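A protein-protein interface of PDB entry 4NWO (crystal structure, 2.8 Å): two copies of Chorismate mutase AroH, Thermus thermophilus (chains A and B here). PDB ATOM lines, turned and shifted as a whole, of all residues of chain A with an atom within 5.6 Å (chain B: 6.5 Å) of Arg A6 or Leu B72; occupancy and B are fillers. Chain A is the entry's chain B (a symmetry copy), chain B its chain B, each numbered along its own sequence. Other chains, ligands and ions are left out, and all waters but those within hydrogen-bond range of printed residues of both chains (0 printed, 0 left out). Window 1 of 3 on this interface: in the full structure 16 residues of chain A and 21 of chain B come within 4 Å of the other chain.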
ATOM      1  N   GLY A   4      -8.013 -21.534  18.755  1.00  0.00           N
ATOM      2  CA  GLY A   4      -8.515 -22.722  18.094  1.00  0.00           C
ATOM      3  C   GLY A   4      -8.686 -22.541  16.600  1.00  0.00           C
ATOM      4  O   GLY A   4      -8.995 -21.451  16.120  1.00  0.00           O
ATOM      5  N   ILE A   5      -8.484 -23.629  15.865  1.00  0.00           N
ATOM      6  CA  ILE A   5      -8.769 -23.684  14.438  1.00  0.00           C
ATOM      7  C   ILE A   5      -9.762 -24.815  14.208  1.00  0.00           C
ATOM      8  O   ILE A   5      -9.508 -25.956  14.598  1.00  0.00           O
ATOM      9  CB  ILE A   5      -7.499 -23.909  13.594  1.00  0.00           C
ATOM     10  CG1 ILE A   5      -6.403 -22.923  14.002  1.00  0.00           C
ATOM     11  CG2 ILE A   5      -7.815 -23.768  12.113  1.00  0.00           C
ATOM     12  CD1 ILE A   5      -5.054 -23.222  13.390  1.00  0.00           C
ATOM     13  N   ARG A   6     -10.896 -24.503  13.592  1.00  0.00           N
ATOM     14  CA  ARG A   6     -11.864 -25.535  13.253  1.00  0.00           C
ATOM     15  C   ARG A   6     -11.697 -25.999  11.816  1.00  0.00           C
ATOM     16  O   ARG A   6     -11.402 -25.209  10.921  1.00  0.00           O
ATOM     17  CB  ARG A   6     -13.286 -25.009  13.471  1.00  0.00           C
ATOM     18  CG  ARG A   6     -13.801 -25.180  14.888  1.00  0.00           C
ATOM     19  CD  ARG A   6     -13.873 -26.642  15.304  1.00  0.00           C
ATOM     20  NE  ARG A   6     -14.426 -27.503  14.260  1.00  0.00           N
ATOM     21  CZ  ARG A   6     -15.712 -27.536  13.920  1.00  0.00           C
ATOM     22  NH1 ARG A   6     -16.124 -28.352  12.962  1.00  0.00           N
ATOM     23  NH2 ARG A   6     -16.587 -26.754  14.539  1.00  0.00           N
ATOM     24  N   GLY A   7     -11.888 -27.295  11.608  1.00  0.00           N
ATOM     25  CA  GLY A   7     -11.996 -27.846  10.275  1.00  0.00           C
ATOM     26  C   GLY A   7     -13.118 -28.859  10.220  1.00  0.00           C
ATOM     27  O   GLY A   7     -13.537 -29.380  11.254  1.00  0.00           O
ATOM     28  N   ALA A   8     -13.601 -29.145   9.016  1.00  0.00           N
ATOM     29  CA  ALA A   8     -14.524 -30.251   8.817  1.00  0.00           C
ATOM     30  C   ALA A   8     -14.466 -30.763   7.385  1.00  0.00           C
ATOM     31  O   ALA A   8     -14.171 -30.011   6.456  1.00  0.00           O
ATOM     32  CB  ALA A   8     -15.943 -29.828   9.173  1.00  0.00           C
ATOM     33  N   MET A  30      -5.840 -26.953   6.524  1.00  0.00           N
ATOM     34  CA  MET A  30      -5.904 -26.104   7.714  1.00  0.00           C
ATOM     35  C   MET A  30      -4.582 -25.397   7.997  1.00  0.00           C
ATOM     36  O   MET A  30      -4.559 -24.209   8.320  1.00  0.00           O
ATOM     37  CB  MET A  30      -6.332 -26.915   8.941  1.00  0.00           C
ATOM     38  CG  MET A  30      -7.791 -27.353   8.930  1.00  0.00           C
ATOM     39  SD  MET A  30      -8.199 -28.490  10.269  1.00  0.00           S
ATOM     40  CE  MET A  30      -8.129 -27.399  11.686  1.00  0.00           C
ATOM     41  N   ARG A  89     -14.582 -33.778  12.142  1.00  0.00           N
ATOM     42  CA  ARG A  89     -14.312 -32.427  12.622  1.00  0.00           C
ATOM     43  C   ARG A  89     -12.980 -32.336  13.355  1.00  0.00           C
ATOM     44  O   ARG A  89     -12.576 -33.265  14.051  1.00  0.00           O
ATOM     45  CB  ARG A  89     -15.439 -31.939  13.537  1.00  0.00           C
ATOM     46  CG  ARG A  89     -16.777 -31.759  12.846  1.00  0.00           C
ATOM     47  CD  ARG A  89     -17.877 -31.438  13.848  1.00  0.00           C
ATOM     48  NE  ARG A  89     -19.102 -30.991  13.188  1.00  0.00           N
ATOM     49  CZ  ARG A  89     -20.061 -31.802  12.757  1.00  0.00           C
ATOM     50  NH1 ARG A  89     -19.936 -33.114  12.900  1.00  0.00           N
ATOM     51  NH2 ARG A  89     -21.162 -31.300  12.212  1.00  0.00           N
ATOM     52  N   VAL A  90     -12.302 -31.204  13.191  1.00  0.00           N
ATOM     53  CA  VAL A  90     -11.012 -30.987  13.833  1.00  0.00           C
ATOM     54  C   VAL A  90     -11.023 -29.684  14.625  1.00  0.00           C
ATOM     55  O   VAL A  90     -11.509 -28.660  14.149  1.00  0.00           O
ATOM     56  CB  VAL A  90      -9.874 -30.939  12.786  1.00  0.00           C
ATOM     57  CG1 VAL A  90      -8.531 -30.702  13.452  1.00  0.00           C
ATOM     58  CG2 VAL A  90      -9.855 -32.213  11.962  1.00  0.00           C
ATOM     59  N   LEU A  91     -10.483 -29.736  15.838  1.00  0.00           N
ATOM     60  CA  LEU A  91     -10.135 -28.532  16.579  1.00  0.00           C
ATOM     61  C   LEU A  91      -8.653 -28.510  16.929  1.00  0.00           C
ATOM     62  O   LEU A  91      -8.213 -29.200  17.849  1.00  0.00           O
ATOM     63  CB  LEU A  91     -10.977 -28.414  17.849  1.00  0.00           C
ATOM     64  CG  LEU A  91     -10.651 -27.210  18.738  1.00  0.00           C
ATOM     65  CD1 LEU A  91     -10.980 -25.917  18.012  1.00  0.00           C
ATOM     66  CD2 LEU A  91     -11.402 -27.294  20.056  1.00  0.00           C
ATOM     67  N   ALA A  92      -7.886 -27.724  16.185  1.00  0.00           N
ATOM     68  CA  ALA A  92      -6.472 -27.536  16.476  1.00  0.00           C
ATOM     69  C   ALA A  92      -6.251 -26.367  17.430  1.00  0.00           C
ATOM     70  O   ALA A  92      -6.779 -25.277  17.218  1.00  0.00           O
ATOM     71  CB  ALA A  92      -5.695 -27.321  15.188  1.00  0.00           C
ATOM     72  N   ARG A 104      -8.162 -18.645  10.096  1.00  0.00           N
ATOM     73  CA  ARG A 104      -8.912 -19.189   8.970  1.00  0.00           C
ATOM     74  C   ARG A 104      -9.343 -20.634   9.204  1.00  0.00           C
ATOM     75  O   ARG A 104      -8.523 -21.538   9.375  1.00  0.00           O
ATOM     76  CB  ARG A 104      -8.087 -19.089   7.685  1.00  0.00           C
ATOM     77  CG  ARG A 104      -7.701 -17.668   7.304  1.00  0.00           C
ATOM     78  N   HIS A 105     -10.657 -20.818   9.195  1.00  0.00           N
ATOM     79  CA  HIS A 105     -11.319 -22.096   9.418  1.00  0.00           C
ATOM     80  C   HIS A 105     -11.660 -22.761   8.081  1.00  0.00           C
ATOM     81  O   HIS A 105     -11.995 -22.079   7.116  1.00  0.00           O
ATOM     82  CB  HIS A 105     -12.549 -21.879  10.293  1.00  0.00           C
ATOM     83  CG  HIS A 105     -12.239 -21.161  11.571  1.00  0.00           C
ATOM     84  ND1 HIS A 105     -11.562 -21.757  12.614  1.00  0.00           N
ATOM     85  CD2 HIS A 105     -12.481 -19.887  11.960  1.00  0.00           C
ATOM     86  CE1 HIS A 105     -11.417 -20.886  13.598  1.00  0.00           C
ATOM     87  NE2 HIS A 105     -11.966 -19.744  13.226  1.00  0.00           N
ATOM     88  N   VAL A 106     -11.572 -24.086   8.021  1.00  0.00           N
ATOM     89  CA  VAL A 106     -11.595 -24.811   6.748  1.00  0.00           C
ATOM     90  C   VAL A 106     -12.678 -25.885   6.660  1.00  0.00           C
ATOM     91  O   VAL A 106     -12.658 -26.868   7.394  1.00  0.00           O
ATOM     92  CB  VAL A 106     -10.239 -25.494   6.477  1.00  0.00           C
ATOM     93  CG1 VAL A 106     -10.286 -26.267   5.167  1.00  0.00           C
ATOM     94  CG2 VAL A 106      -9.118 -24.469   6.463  1.00  0.00           C
ATOM     95  N   TYR A 107     -13.625 -25.679   5.749  1.00  0.00           N
ATOM     96  CA  TYR A 107     -14.756 -26.584   5.576  1.00  0.00           C
ATOM     97  C   TYR A 107     -14.781 -27.134   4.145  1.00  0.00           C
ATOM     98  O   TYR A 107     -14.958 -26.380   3.189  1.00  0.00           O
ATOM     99  CB  TYR A 107     -16.060 -25.849   5.884  1.00  0.00           C
ATOM    100  CG  TYR A 107     -16.272 -25.576   7.356  1.00  0.00           C
ATOM    101  CD1 TYR A 107     -15.692 -24.468   7.960  1.00  0.00           C
ATOM    102  CD2 TYR A 107     -17.047 -26.418   8.140  1.00  0.00           C
ATOM    103  CE1 TYR A 107     -15.880 -24.202   9.303  1.00  0.00           C
ATOM    104  CE2 TYR A 107     -17.238 -26.161   9.488  1.00  0.00           C
ATOM    105  CZ  TYR A 107     -16.652 -25.051  10.062  1.00  0.00           C
ATOM    106  OH  TYR A 107     -16.834 -24.792  11.399  1.00  0.00           O
ATOM    107  N   ALA B  44     -11.212 -21.239  22.560  1.00  0.00           N
ATOM    108  CA  ALA B  44     -12.132 -22.248  22.041  1.00  0.00           C
ATOM    109  C   ALA B  44     -13.157 -22.608  23.112  1.00  0.00           C
ATOM    110  O   ALA B  44     -12.953 -22.320  24.290  1.00  0.00           O
ATOM    111  CB  ALA B  44     -11.376 -23.491  21.591  1.00  0.00           C
ATOM    112  N   VAL B  45     -14.259 -23.231  22.703  1.00  0.00           N
ATOM    113  CA  VAL B  45     -15.229 -23.771  23.653  1.00  0.00           C
ATOM    114  C   VAL B  45     -15.651 -25.187  23.264  1.00  0.00           C
ATOM    115  O   VAL B  45     -16.013 -25.440  22.116  1.00  0.00           O
ATOM    116  CB  VAL B  45     -16.485 -22.873  23.753  1.00  0.00           C
ATOM    117  CG1 VAL B  45     -17.441 -23.411  24.797  1.00  0.00           C
ATOM    118  CG2 VAL B  45     -16.105 -21.431  24.070  1.00  0.00           C
ATOM    119  N   ILE B  46     -15.605 -26.101  24.228  1.00  0.00           N
ATOM    120  CA  ILE B  46     -16.012 -27.487  24.014  1.00  0.00           C
ATOM    121  C   ILE B  46     -17.257 -27.867  24.820  1.00  0.00           C
ATOM    122  O   ILE B  46     -17.363 -27.538  26.003  1.00  0.00           O
ATOM    123  CB  ILE B  46     -14.870 -28.457  24.376  1.00  0.00           C
ATOM    124  CG1 ILE B  46     -13.611 -28.120  23.577  1.00  0.00           C
ATOM    125  CG2 ILE B  46     -15.293 -29.900  24.141  1.00  0.00           C
ATOM    126  CD1 ILE B  46     -12.372 -28.834  24.066  1.00  0.00           C
ATOM    127  N   PHE B  47     -18.194 -28.561  24.182  1.00  0.00           N
ATOM    128  CA  PHE B  47     -19.409 -28.991  24.864  1.00  0.00           C
ATOM    129  C   PHE B  47     -19.455 -30.508  24.930  1.00  0.00           C
ATOM    130  O   PHE B  47     -18.916 -31.187  24.056  1.00  0.00           O
ATOM    131  CB  PHE B  47     -20.664 -28.497  24.135  1.00  0.00           C
ATOM    132  CG  PHE B  47     -20.729 -27.011  23.947  1.00  0.00           C
ATOM    133  CD1 PHE B  47     -20.171 -26.415  22.828  1.00  0.00           C
ATOM    134  CD2 PHE B  47     -21.382 -26.212  24.867  1.00  0.00           C
ATOM    135  CE1 PHE B  47     -20.242 -25.045  22.644  1.00  0.00           C
ATOM    136  CE2 PHE B  47     -21.457 -24.841  24.690  1.00  0.00           C
ATOM    137  CZ  PHE B  47     -20.887 -24.258  23.576  1.00  0.00           C
ATOM    138  N   PRO B  58     -25.560 -28.015  20.992  1.00  0.00           N
ATOM    139  CA  PRO B  58     -25.279 -26.949  21.966  1.00  0.00           C
ATOM    140  C   PRO B  58     -24.511 -25.783  21.345  1.00  0.00           C
ATOM    141  O   PRO B  58     -24.678 -24.635  21.757  1.00  0.00           O
ATOM    142  CB  PRO B  58     -24.434 -27.649  23.032  1.00  0.00           C
ATOM    143  CG  PRO B  58     -24.732 -29.089  22.881  1.00  0.00           C
ATOM    144  CD  PRO B  58     -25.088 -29.332  21.456  1.00  0.00           C
ATOM    145  N   ALA B  59     -23.685 -26.098  20.354  1.00  0.00           N
ATOM    146  CA  ALA B  59     -22.854 -25.129  19.643  1.00  0.00           C
ATOM    147  C   ALA B  59     -23.703 -24.092  18.911  1.00  0.00           C
ATOM    148  O   ALA B  59     -23.277 -22.957  18.703  1.00  0.00           O
ATOM    149  CB  ALA B  59     -21.935 -25.843  18.666  1.00  0.00           C
ATOM    150  N   GLU B  60     -24.904 -24.501  18.522  1.00  0.00           N
ATOM    151  CA  GLU B  60     -25.878 -23.631  17.870  1.00  0.00           C
ATOM    152  C   GLU B  60     -26.308 -22.471  18.770  1.00  0.00           C
ATOM    153  O   GLU B  60     -26.492 -21.348  18.303  1.00  0.00           O
ATOM    154  CB  GLU B  60     -27.104 -24.439  17.438  1.00  0.00           C
ATOM    155  N   ALA B  62     -24.469 -21.069  21.164  1.00  0.00           N
ATOM    156  CA  ALA B  62     -23.365 -20.114  21.221  1.00  0.00           C
ATOM    157  C   ALA B  62     -23.380 -19.149  20.036  1.00  0.00           C
ATOM    158  O   ALA B  62     -23.053 -17.973  20.182  1.00  0.00           O
ATOM    159  CB  ALA B  62     -22.036 -20.848  21.281  1.00  0.00           C
ATOM    160  N   ARG B  63     -23.744 -19.650  18.860  1.00  0.00           N
ATOM    161  CA  ARG B  63     -23.880 -18.803  17.679  1.00  0.00           C
ATOM    162  C   ARG B  63     -25.092 -17.872  17.746  1.00  0.00           C
ATOM    163  O   ARG B  63     -25.137 -16.854  17.058  1.00  0.00           O
ATOM    164  CB  ARG B  63     -23.962 -19.668  16.419  1.00  0.00           C
ATOM    165  N   MET B  67     -21.186 -15.823  18.856  1.00  0.00           N
ATOM    166  CA  MET B  67     -19.884 -16.485  19.000  1.00  0.00           C
ATOM    167  C   MET B  67     -19.426 -17.098  17.674  1.00  0.00           C
ATOM    168  O   MET B  67     -18.770 -18.139  17.658  1.00  0.00           O
ATOM    169  CB  MET B  67     -19.915 -17.554  20.096  1.00  0.00           C
ATOM    170  CG  MET B  67     -20.100 -17.005  21.499  1.00  0.00           C
ATOM    171  SD  MET B  67     -19.700 -18.225  22.766  1.00  0.00           S
ATOM    172  CE  MET B  67     -19.910 -17.250  24.252  1.00  0.00           C
ATOM    173  N   HIS B  68     -19.781 -16.450  16.571  1.00  0.00           N
ATOM    174  CA  HIS B  68     -19.392 -16.886  15.231  1.00  0.00           C
ATOM    175  C   HIS B  68     -17.885 -17.039  15.020  1.00  0.00           C
ATOM    176  O   HIS B  68     -17.447 -17.982  14.359  1.00  0.00           O
ATOM    177  CB  HIS B  68     -19.941 -15.898  14.199  1.00  0.00           C
ATOM    178  CG  HIS B  68     -21.436 -15.866  14.128  1.00  0.00           C
ATOM    179  ND1 HIS B  68     -22.205 -15.148  15.018  1.00  0.00           N
ATOM    180  CD2 HIS B  68     -22.303 -16.456  13.271  1.00  0.00           C
ATOM    181  CE1 HIS B  68     -23.482 -15.300  14.715  1.00  0.00           C
ATOM    182  NE2 HIS B  68     -23.569 -16.088  13.658  1.00  0.00           N
ATOM    183  N   VAL B  70     -15.683 -17.561  17.310  1.00  0.00           N
ATOM    184  CA  VAL B  70     -15.157 -18.511  18.288  1.00  0.00           C
ATOM    185  C   VAL B  70     -15.302 -19.964  17.833  1.00  0.00           C
ATOM    186  O   VAL B  70     -16.387 -20.397  17.447  1.00  0.00           O
ATOM    187  CB  VAL B  70     -15.852 -18.344  19.651  1.00  0.00           C
ATOM    188  CG1 VAL B  70     -15.236 -19.280  20.682  1.00  0.00           C
ATOM    189  CG2 VAL B  70     -15.765 -16.897  20.115  1.00  0.00           C
ATOM    190  N   PRO B  71     -14.193 -20.719  17.870  1.00  0.00           N
ATOM    191  CA  PRO B  71     -14.193 -22.136  17.482  1.00  0.00           C
ATOM    192  C   PRO B  71     -14.899 -23.031  18.497  1.00  0.00           C
ATOM    193  O   PRO B  71     -14.588 -22.994  19.688  1.00  0.00           O
ATOM    194  CB  PRO B  71     -12.706 -22.501  17.405  1.00  0.00           C
ATOM    195  CG  PRO B  71     -11.936 -21.271  17.673  1.00  0.00           C
ATOM    196  CD  PRO B  71     -12.843 -20.180  18.105  1.00  0.00           C
ATOM    197  N   LEU B  72     -15.840 -23.836  18.015  1.00  0.00           N
ATOM    198  CA  LEU B  72     -16.686 -24.643  18.885  1.00  0.00           C
ATOM    199  C   LEU B  72     -16.575 -26.116  18.520  1.00  0.00           C
ATOM    200  O   LEU B  72     -16.402 -26.466  17.352  1.00  0.00           O
ATOM    201  CB  LEU B  72     -18.147 -24.194  18.786  1.00  0.00           C
ATOM    202  CG  LEU B  72     -18.476 -22.713  18.987  1.00  0.00           C
ATOM    203  CD1 LEU B  72     -19.950 -22.456  18.722  1.00  0.00           C
ATOM    204  CD2 LEU B  72     -18.097 -22.247  20.385  1.00  0.00           C
ATOM    205  N   LEU B  73     -16.675 -26.979  19.525  1.00  0.00           N
ATOM    206  CA  LEU B  73     -16.667 -28.415  19.293  1.00  0.00           C
ATOM    207  C   LEU B  73     -17.557 -29.099  20.323  1.00  0.00           C
ATOM    208  O   LEU B  73     -17.639 -28.661  21.469  1.00  0.00           O
ATOM    209  CB  LEU B  73     -15.238 -28.964  19.344  1.00  0.00           C
ATOM    210  CG  LEU B  73     -15.017 -30.349  18.729  1.00  0.00           C
ATOM    211  CD1 LEU B  73     -15.113 -30.258  17.218  1.00  0.00           C
ATOM    212  CD2 LEU B  73     -13.667 -30.912  19.139  1.00  0.00           C
ATOM    213  N   SER B  74     -18.236 -30.161  19.905  1.00  0.00           N
ATOM    214  CA  SER B  74     -19.109 -30.902  20.805  1.00  0.00           C
ATOM    215  C   SER B  74     -18.846 -32.402  20.735  1.00  0.00           C
ATOM    216  O   SER B  74     -18.423 -32.924  19.704  1.00  0.00           O
ATOM    217  CB  SER B  74     -20.574 -30.608  20.486  1.00  0.00           C
ATOM    218  OG  SER B  74     -20.848 -30.825  19.114  1.00  0.00           O
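Printed residues of chain B that touch a printed residue of chain A: Pro B71, Leu B72 and Leu B73.
Hydrophobic or aromatic side chains of chain B that line the printed part of chain A: Pro B71 and Leu B73.
Among the printed residues, no Asp or Glu carboxylate lies within 4 Å of a Lys or Arg side-chain nitrogen of the other chain.
NH2 of Arg A6 sits at hydrogen-bond distance from O of Leu B72.
Printed residues of chain B within 4 Å of Gly A4: Pro B71.
Arg A6 touches just these residues of chain B: Pro B71 and Leu B72.
Of the printed residues of chain B, Leu A91 touches Pro B71 (3.9 Å) and Leu B73 (3.9 Å).
Ala B44 touches none of the printed residues of chain A.
Arg B63 touches none of the printed residues of chain A.
Of the printed residues of chain A, Pro B71 touches Gly A4 (3.3 Å), Arg A6 (3.8 Å) and Leu A91 (3.9 Å).
Leu B72 touches one residue of chain A.
Printed residues of chain A within 4 Å of Leu B73: Leu A91.
The nearest residue of chain A that does not touch Leu B72 is Leu A91 (5.3 Å).
The nearest printed residue of chain A that does not touch Leu B73 is Arg A89 (4.1 Å).
Among the printed residues, pairs that only touch across the chains: Gly A4 with Pro B71 (3.3 Å), Arg A6 with Pro B71 (3.8 Å), Leu A91 with Pro B71 (3.9 Å) and Leu A91 with Leu B73 (3.9 Å).
No position is printed for both chains.
The backbone carbonyl oxygen (O) of Val B45 lies within hydrogen-bond range of the backbone NH (N) of Leu B73 (3.1 Å).
The backbone NH (N) of Arg A6 sits at hydrogen-bond distance from a ring nitrogen (ND1) of His A105, at 3.0 Å.
The backbone carbonyl oxygen (O) of Val A90 lies within hydrogen-bond range of the guanidinium group (NE) of Arg A6, 3.1 Å away.
The backbone carbonyl oxygen of Arg A6 lies within hydrogen-bond range of the backbone NH of Val A106.
O of Leu B73 sits at hydrogen-bond distance from N of Phe B47 (2.8 Å).
The backbone carbonyl oxygen (O) of Pro B71 sits at hydrogen-bond distance from the backbone NH (N) of Val B45, 3.0 Å away.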
